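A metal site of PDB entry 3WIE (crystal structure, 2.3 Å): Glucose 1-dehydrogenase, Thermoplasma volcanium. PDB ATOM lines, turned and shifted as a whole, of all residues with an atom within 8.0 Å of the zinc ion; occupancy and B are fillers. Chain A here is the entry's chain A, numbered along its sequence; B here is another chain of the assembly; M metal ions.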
ATOM      1  N   ARG A  94       0.316 -22.053   7.496  1.00  0.00           N
ATOM      2  CA  ARG A  94      -0.254 -20.744   7.784  1.00  0.00           C
ATOM      3  C   ARG A  94      -1.153 -20.297   6.691  1.00  0.00           C
ATOM      4  O   ARG A  94      -0.748 -20.276   5.500  1.00  0.00           O
ATOM      5  CB  ARG A  94       0.790 -19.681   7.955  1.00  0.00           C
ATOM      6  CG  ARG A  94       0.219 -18.456   8.592  1.00  0.00           C
ATOM      7  CD  ARG A  94       1.238 -17.350   8.808  1.00  0.00           C
ATOM      8  NE  ARG A  94       1.971 -17.559  10.019  1.00  0.00           N
ATOM      9  CZ  ARG A  94       2.627 -16.606  10.680  1.00  0.00           C
ATOM     10  NH1 ARG A  94       2.647 -15.334  10.251  1.00  0.00           N
ATOM     11  NH2 ARG A  94       3.285 -16.931  11.773  1.00  0.00           N
ATOM     12  N   ARG A  95      -2.367 -19.866   7.092  1.00  0.00           N
ATOM     13  CA  ARG A  95      -3.409 -19.467   6.138  1.00  0.00           C
ATOM     14  C   ARG A  95      -3.642 -17.997   6.295  1.00  0.00           C
ATOM     15  O   ARG A  95      -3.606 -17.483   7.389  1.00  0.00           O
ATOM     16  CB  ARG A  95      -4.729 -20.232   6.396  1.00  0.00           C
ATOM     17  CG  ARG A  95      -4.522 -21.699   6.697  1.00  0.00           C
ATOM     18  CD  ARG A  95      -4.023 -22.339   5.464  1.00  0.00           C
ATOM     19  NE  ARG A  95      -3.580 -23.724   5.512  1.00  0.00           N
ATOM     20  CZ  ARG A  95      -4.174 -24.734   4.914  1.00  0.00           C
ATOM     21  NH1 ARG A  95      -5.410 -24.629   4.430  1.00  0.00           N
ATOM     22  NH2 ARG A  95      -3.571 -25.904   4.866  1.00  0.00           N
ATOM     23  N   PRO A  96      -3.858 -17.292   5.173  1.00  0.00           N
ATOM     24  CA  PRO A  96      -3.879 -15.823   5.203  1.00  0.00           C
ATOM     25  C   PRO A  96      -5.168 -15.218   5.768  1.00  0.00           C
ATOM     26  O   PRO A  96      -6.254 -15.793   5.614  1.00  0.00           O
ATOM     27  CB  PRO A  96      -3.796 -15.441   3.717  1.00  0.00           C
ATOM     28  CG  PRO A  96      -4.376 -16.627   2.968  1.00  0.00           C
ATOM     29  CD  PRO A  96      -4.018 -17.836   3.824  1.00  0.00           C
ATOM     30  N   GLY A  97      -5.054 -14.054   6.409  1.00  0.00           N
ATOM     31  CA  GLY A  97      -6.175 -13.206   6.735  1.00  0.00           C
ATOM     32  C   GLY A  97      -6.371 -12.138   5.698  1.00  0.00           C
ATOM     33  O   GLY A  97      -6.375 -12.433   4.505  1.00  0.00           O
ATOM     34  N   LYS A  98      -6.565 -10.895   6.142  1.00  0.00           N
ATOM     35  CA  LYS A  98      -6.944  -9.792   5.222  1.00  0.00           C
ATOM     36  C   LYS A  98      -5.900  -8.710   5.107  1.00  0.00           C
ATOM     37  O   LYS A  98      -6.063  -7.844   4.276  1.00  0.00           O
ATOM     38  CB  LYS A  98      -8.194  -9.100   5.759  1.00  0.00           C
ATOM     39  CG  LYS A  98      -9.339 -10.033   6.122  1.00  0.00           C
ATOM     40  CD  LYS A  98     -10.296 -10.320   4.966  1.00  0.00           C
ATOM     41  CE  LYS A  98     -11.733 -10.514   5.480  1.00  0.00           C
ATOM     42  NZ  LYS A  98     -12.766 -10.228   4.446  1.00  0.00           N
ATOM     43  N   CYS A  99      -4.775  -8.831   5.799  1.00  0.00           N
ATOM     44  CA  CYS A  99      -3.870  -7.716   5.882  1.00  0.00           C
ATOM     45  C   CYS A  99      -3.249  -7.434   4.542  1.00  0.00           C
ATOM     46  O   CYS A  99      -3.518  -8.054   3.511  1.00  0.00           O
ATOM     47  CB  CYS A  99      -2.776  -7.958   6.907  1.00  0.00           C
ATOM     48  SG  CYS A  99      -1.732  -9.401   6.640  1.00  0.00           S
ATOM     49  N   VAL A 100      -2.418  -6.406   4.552  1.00  0.00           N
ATOM     50  CA  VAL A 100      -1.650  -6.092   3.351  1.00  0.00           C
ATOM     51  C   VAL A 100      -0.646  -7.206   2.919  1.00  0.00           C
ATOM     52  O   VAL A 100      -0.470  -7.421   1.726  1.00  0.00           O
ATOM     53  CB  VAL A 100      -1.000  -4.697   3.510  1.00  0.00           C
ATOM     54  CG1 VAL A 100       0.143  -4.699   4.520  1.00  0.00           C
ATOM     55  CG2 VAL A 100      -0.563  -4.132   2.202  1.00  0.00           C
ATOM     56  N   ASN A 101      -0.010  -7.871   3.893  1.00  0.00           N
ATOM     57  CA  ASN A 101       0.874  -9.032   3.652  1.00  0.00           C
ATOM     58  C   ASN A 101       0.142 -10.364   3.394  1.00  0.00           C
ATOM     59  O   ASN A 101       0.418 -11.078   2.434  1.00  0.00           O
ATOM     60  CB  ASN A 101       1.897  -9.151   4.801  1.00  0.00           C
ATOM     61  CG  ASN A 101       2.985  -8.092   4.666  1.00  0.00           C
ATOM     62  OD1 ASN A 101       3.779  -8.188   3.760  1.00  0.00           O
ATOM     63  ND2 ASN A 101       2.945  -7.046   5.480  1.00  0.00           N
ATOM     64  N   CYS A 102      -0.822 -10.644   4.243  1.00  0.00           N
ATOM     65  CA  CYS A 102      -1.682 -11.808   4.119  1.00  0.00           C
ATOM     66  C   CYS A 102      -2.315 -11.886   2.678  1.00  0.00           C
ATOM     67  O   CYS A 102      -2.316 -12.945   2.061  1.00  0.00           O
ATOM     68  CB  CYS A 102      -2.666 -11.835   5.377  1.00  0.00           C
ATOM     69  SG  CYS A 102      -2.091 -12.448   6.989  1.00  0.00           S
ATOM     70  N   ARG A 103      -2.692 -10.757   2.076  1.00  0.00           N
ATOM     71  CA  ARG A 103      -3.454 -10.736   0.807  1.00  0.00           C
ATOM     72  C   ARG A 103      -2.624 -10.893  -0.442  1.00  0.00           C
ATOM     73  O   ARG A 103      -3.157 -11.081  -1.560  1.00  0.00           O
ATOM     74  CB  ARG A 103      -4.343  -9.457   0.724  1.00  0.00           C
ATOM     75  CG  ARG A 103      -3.549  -8.173   0.426  1.00  0.00           C
ATOM     76  CD  ARG A 103      -4.410  -6.896   0.441  1.00  0.00           C
ATOM     77  NE  ARG A 103      -4.882  -6.584   1.789  1.00  0.00           N
ATOM     78  CZ  ARG A 103      -5.427  -5.444   2.147  1.00  0.00           C
ATOM     79  NH1 ARG A 103      -5.845  -5.281   3.369  1.00  0.00           N
ATOM     80  NH2 ARG A 103      -5.597  -4.499   1.269  1.00  0.00           N
ATOM     81  N   ARG A 106       1.760 -13.536   1.570  1.00  0.00           N
ATOM     82  CA  ARG A 106       2.823 -13.391   2.493  1.00  0.00           C
ATOM     83  C   ARG A 106       2.293 -13.289   3.891  1.00  0.00           C
ATOM     84  O   ARG A 106       2.746 -12.469   4.692  1.00  0.00           O
ATOM     85  CB  ARG A 106       3.674 -12.204   2.149  1.00  0.00           C
ATOM     86  CG  ARG A 106       4.334 -12.269   0.762  1.00  0.00           C
ATOM     87  CD  ARG A 106       5.242 -13.506   0.609  1.00  0.00           C
ATOM     88  NE  ARG A 106       6.140 -13.802   1.743  1.00  0.00           N
ATOM     89  CZ  ARG A 106       7.481 -13.717   1.696  1.00  0.00           C
ATOM     90  NH1 ARG A 106       8.119 -13.281   0.633  1.00  0.00           N
ATOM     91  NH2 ARG A 106       8.227 -14.067   2.716  1.00  0.00           N
ATOM     92  N   GLN A 107       1.412 -14.240   4.227  1.00  0.00           N
ATOM     93  CA  GLN A 107       0.959 -14.422   5.593  1.00  0.00           C
ATOM     94  C   GLN A 107       2.046 -14.808   6.646  1.00  0.00           C
ATOM     95  O   GLN A 107       1.886 -14.577   7.874  1.00  0.00           O
ATOM     96  CB  GLN A 107      -0.219 -15.435   5.573  1.00  0.00           C
ATOM     97  CG  GLN A 107       0.061 -16.859   5.191  1.00  0.00           C
ATOM     98  CD  GLN A 107      -0.155 -17.109   3.736  1.00  0.00           C
ATOM     99  OE1 GLN A 107      -0.137 -16.219   2.903  1.00  0.00           O
ATOM    100  NE2 GLN A 107      -0.445 -18.335   3.410  1.00  0.00           N
ATOM    101  N   ASP A 108       3.176 -15.286   6.177  1.00  0.00           N
ATOM    102  CA  ASP A 108       4.331 -15.496   7.032  1.00  0.00           C
ATOM    103  C   ASP A 108       4.759 -14.174   7.657  1.00  0.00           C
ATOM    104  O   ASP A 108       5.184 -14.147   8.763  1.00  0.00           O
ATOM    105  CB  ASP A 108       5.499 -16.148   6.295  1.00  0.00           C
ATOM    106  CG  ASP A 108       5.882 -15.436   5.057  1.00  0.00           C
ATOM    107  OD1 ASP A 108       5.071 -15.235   4.191  1.00  0.00           O
ATOM    108  OD2 ASP A 108       7.025 -15.084   4.917  1.00  0.00           O
ATOM    109  N   ASN A 109       4.579 -13.099   6.911  1.00  0.00           N
ATOM    110  CA  ASN A 109       4.753 -11.719   7.324  1.00  0.00           C
ATOM    111  C   ASN A 109       3.488 -10.922   7.765  1.00  0.00           C
ATOM    112  O   ASN A 109       3.383  -9.771   7.517  1.00  0.00           O
ATOM    113  CB  ASN A 109       5.494 -10.967   6.236  1.00  0.00           C
ATOM    114  CG  ASN A 109       6.873 -11.510   5.997  1.00  0.00           C
ATOM    115  OD1 ASN A 109       7.512 -11.934   6.906  1.00  0.00           O
ATOM    116  ND2 ASN A 109       7.314 -11.486   4.796  1.00  0.00           N
ATOM    117  N   CYS A 110       2.506 -11.573   8.358  1.00  0.00           N
ATOM    118  CA  CYS A 110       1.241 -10.909   8.639  1.00  0.00           C
ATOM    119  C   CYS A 110       1.462  -9.676   9.502  1.00  0.00           C
ATOM    120  O   CYS A 110       2.250  -9.692  10.451  1.00  0.00           O
ATOM    121  CB  CYS A 110       0.270 -11.874   9.326  1.00  0.00           C
ATOM    122  SG  CYS A 110      -1.114 -11.065  10.177  1.00  0.00           S
ATOM    123  N   SER A 111       0.754  -8.596   9.161  1.00  0.00           N
ATOM    124  CA  SER A 111       0.945  -7.292   9.818  1.00  0.00           C
ATOM    125  C   SER A 111       0.174  -7.183  11.133  1.00  0.00           C
ATOM    126  O   SER A 111       0.430  -6.307  11.909  1.00  0.00           O
ATOM    127  CB  SER A 111       0.487  -6.169   8.894  1.00  0.00           C
ATOM    128  OG  SER A 111       1.332  -6.079   7.744  1.00  0.00           O
ATOM    129  N   ILE A 112      -0.707  -8.140  11.387  1.00  0.00           N
ATOM    130  CA  ILE A 112      -1.584  -8.136  12.522  1.00  0.00           C
ATOM    131  C   ILE A 112      -1.240  -9.195  13.540  1.00  0.00           C
ATOM    132  O   ILE A 112      -1.302  -8.955  14.735  1.00  0.00           O
ATOM    133  CB  ILE A 112      -3.031  -8.281  12.058  1.00  0.00           C
ATOM    134  CG1 ILE A 112      -3.416  -7.061  11.210  1.00  0.00           C
ATOM    135  CG2 ILE A 112      -4.000  -8.369  13.249  1.00  0.00           C
ATOM    136  CD1 ILE A 112      -4.771  -7.234  10.523  1.00  0.00           C
ATOM    137  N   GLY A 113      -0.805 -10.357  13.082  1.00  0.00           N
ATOM    138  CA  GLY A 113      -0.758 -11.560  13.923  1.00  0.00           C
ATOM    139  C   GLY A 113      -2.135 -12.155  14.078  1.00  0.00           C
ATOM    140  O   GLY A 113      -3.035 -11.936  13.238  1.00  0.00           O
ATOM    141  N   ASP A 114      -2.307 -12.942  15.146  1.00  0.00           N
ATOM    142  CA  ASP A 114      -3.606 -13.447  15.534  1.00  0.00           C
ATOM    143  C   ASP A 114      -4.545 -12.317  15.846  1.00  0.00           C
ATOM    144  O   ASP A 114      -4.153 -11.401  16.533  1.00  0.00           O
ATOM    145  CB  ASP A 114      -3.482 -14.462  16.674  1.00  0.00           C
ATOM    146  CG  ASP A 114      -2.986 -15.828  16.157  1.00  0.00           C
ATOM    147  OD1 ASP A 114      -3.747 -16.539  15.399  1.00  0.00           O
ATOM    148  OD2 ASP A 114      -1.821 -16.140  16.472  1.00  0.00           O
ATOM    149  N   PRO A 115      -5.793 -12.370  15.358  1.00  0.00           N
ATOM    150  CA  PRO A 115      -6.482 -13.460  14.651  1.00  0.00           C
ATOM    151  C   PRO A 115      -6.521 -13.320  13.114  1.00  0.00           C
ATOM    152  O   PRO A 115      -7.339 -13.969  12.445  1.00  0.00           O
ATOM    153  CB  PRO A 115      -7.902 -13.353  15.199  1.00  0.00           C
ATOM    154  CG  PRO A 115      -8.067 -11.900  15.470  1.00  0.00           C
ATOM    155  CD  PRO A 115      -6.716 -11.258  15.610  1.00  0.00           C
ATOM    156  N   ASP A 116      -5.652 -12.514  12.542  1.00  0.00           N
ATOM    157  CA  ASP A 116      -5.681 -12.392  11.102  1.00  0.00           C
ATOM    158  C   ASP A 116      -5.286 -13.727  10.465  1.00  0.00           C
ATOM    159  O   ASP A 116      -6.017 -14.310   9.681  1.00  0.00           O
ATOM    160  CB  ASP A 116      -4.801 -11.250  10.622  1.00  0.00           C
ATOM    161  CG  ASP A 116      -5.246 -10.731   9.282  1.00  0.00           C
ATOM    162  OD1 ASP A 116      -6.470 -10.758   8.971  1.00  0.00           O
ATOM    163  OD2 ASP A 116      -4.381 -10.310   8.509  1.00  0.00           O
ATOM    164  N   LYS A 117      -4.147 -14.238  10.857  1.00  0.00           N
ATOM    165  CA  LYS A 117      -3.597 -15.415  10.223  1.00  0.00           C
ATOM    166  C   LYS A 117      -3.939 -16.570  11.146  1.00  0.00           C
ATOM    167  O   LYS A 117      -4.256 -16.342  12.302  1.00  0.00           O
ATOM    168  CB  LYS A 117      -2.100 -15.163   9.922  1.00  0.00           C
ATOM    169  CG  LYS A 117      -1.016 -15.600  10.895  1.00  0.00           C
ATOM    170  CD  LYS A 117      -1.068 -15.152  12.330  1.00  0.00           C
ATOM    171  CE  LYS A 117       0.155 -15.705  13.058  1.00  0.00           C
ATOM    172  NZ  LYS A 117      -0.092 -16.324  14.378  1.00  0.00           N
ATOM    173  N   HIS A 118      -3.972 -17.784  10.600  1.00  0.00           N
ATOM    174  CA  HIS A 118      -4.183 -18.990  11.406  1.00  0.00           C
ATOM    175  C   HIS A 118      -3.232 -20.097  10.938  1.00  0.00           C
ATOM    176  O   HIS A 118      -2.834 -20.171   9.726  1.00  0.00           O
ATOM    177  CB  HIS A 118      -5.630 -19.489  11.275  1.00  0.00           C
ATOM    178  CG  HIS A 118      -6.627 -18.533  11.822  1.00  0.00           C
ATOM    179  ND1 HIS A 118      -7.302 -17.632  11.030  1.00  0.00           N
ATOM    180  CD2 HIS A 118      -6.985 -18.269  13.094  1.00  0.00           C
ATOM    181  CE1 HIS A 118      -8.073 -16.874  11.787  1.00  0.00           C
ATOM    182  NE2 HIS A 118      -7.898 -17.243  13.052  1.00  0.00           N
ATOM    183  N   ASN B 268       4.308  -6.159  14.576  1.00  0.00           N
ATOM    184  CA  ASN B 268       4.731  -7.070  13.554  1.00  0.00           C
ATOM    185  C   ASN B 268       5.397  -6.306  12.459  1.00  0.00           C
ATOM    186  O   ASN B 268       4.862  -5.263  11.997  1.00  0.00           O
ATOM    187  CB  ASN B 268       3.533  -7.778  12.967  1.00  0.00           C
ATOM    188  CG  ASN B 268       3.057  -8.896  13.854  1.00  0.00           C
ATOM    189  OD1 ASN B 268       3.051 -10.029  13.452  1.00  0.00           O
ATOM    190  ND2 ASN B 268       2.667  -8.567  15.065  1.00  0.00           N
HETATM  191 ZN    ZN M   1      -2.476 -10.818   7.937  1.00  0.00          ZN
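The side-chain sulfur (SG) of Cys 102 lies close to the backbone NH (N) of Gly 97 (3.4 Å). N of Lys 98 lies within hydrogen-bond range of OD1 of Asp 116, 2.8 Å away. SG of Cys 99 sits close to N of Ser 111, at 3.6 Å. The side-chain sulfur (SG) of Cys 99 sits close to the backbone NH (N) of Asn 101 (3.6 Å). NE of Arg 103 sits at hydrogen-bond distance from O of Cys 99 (2.6 Å). The backbone NH (N) of Ile 112 lies close to the side-chain sulfur (SG) of Cys 110, 3.2 Å away. The side-chain sulfur (SG) of Cys 110 lies close to the backbone NH (N) of Gly 113 (3.0 Å). The backbone carbonyl oxygen of Cys 110 sits close to the side-chain amide oxygen of Asn 268 of chain B, 3.1 Å away.
Of the 24 residues printed, 4 come within 4 Å of the zinc ion. Along chain A the residues within 4 Å of the zinc ion span positions 99 to 116. The nearest printed residue that does not touch the zinc ion is Ser 111 (4.1 Å).
The zinc ion is bound by SG of Cys 102 (1.9 Å), OD2 of Asp 116 (2.1 Å), SG of Cys 99 (2.1 Å) and SG of Cys 110 (2.6 Å). The zinc ion has four donor atoms within binding distance.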
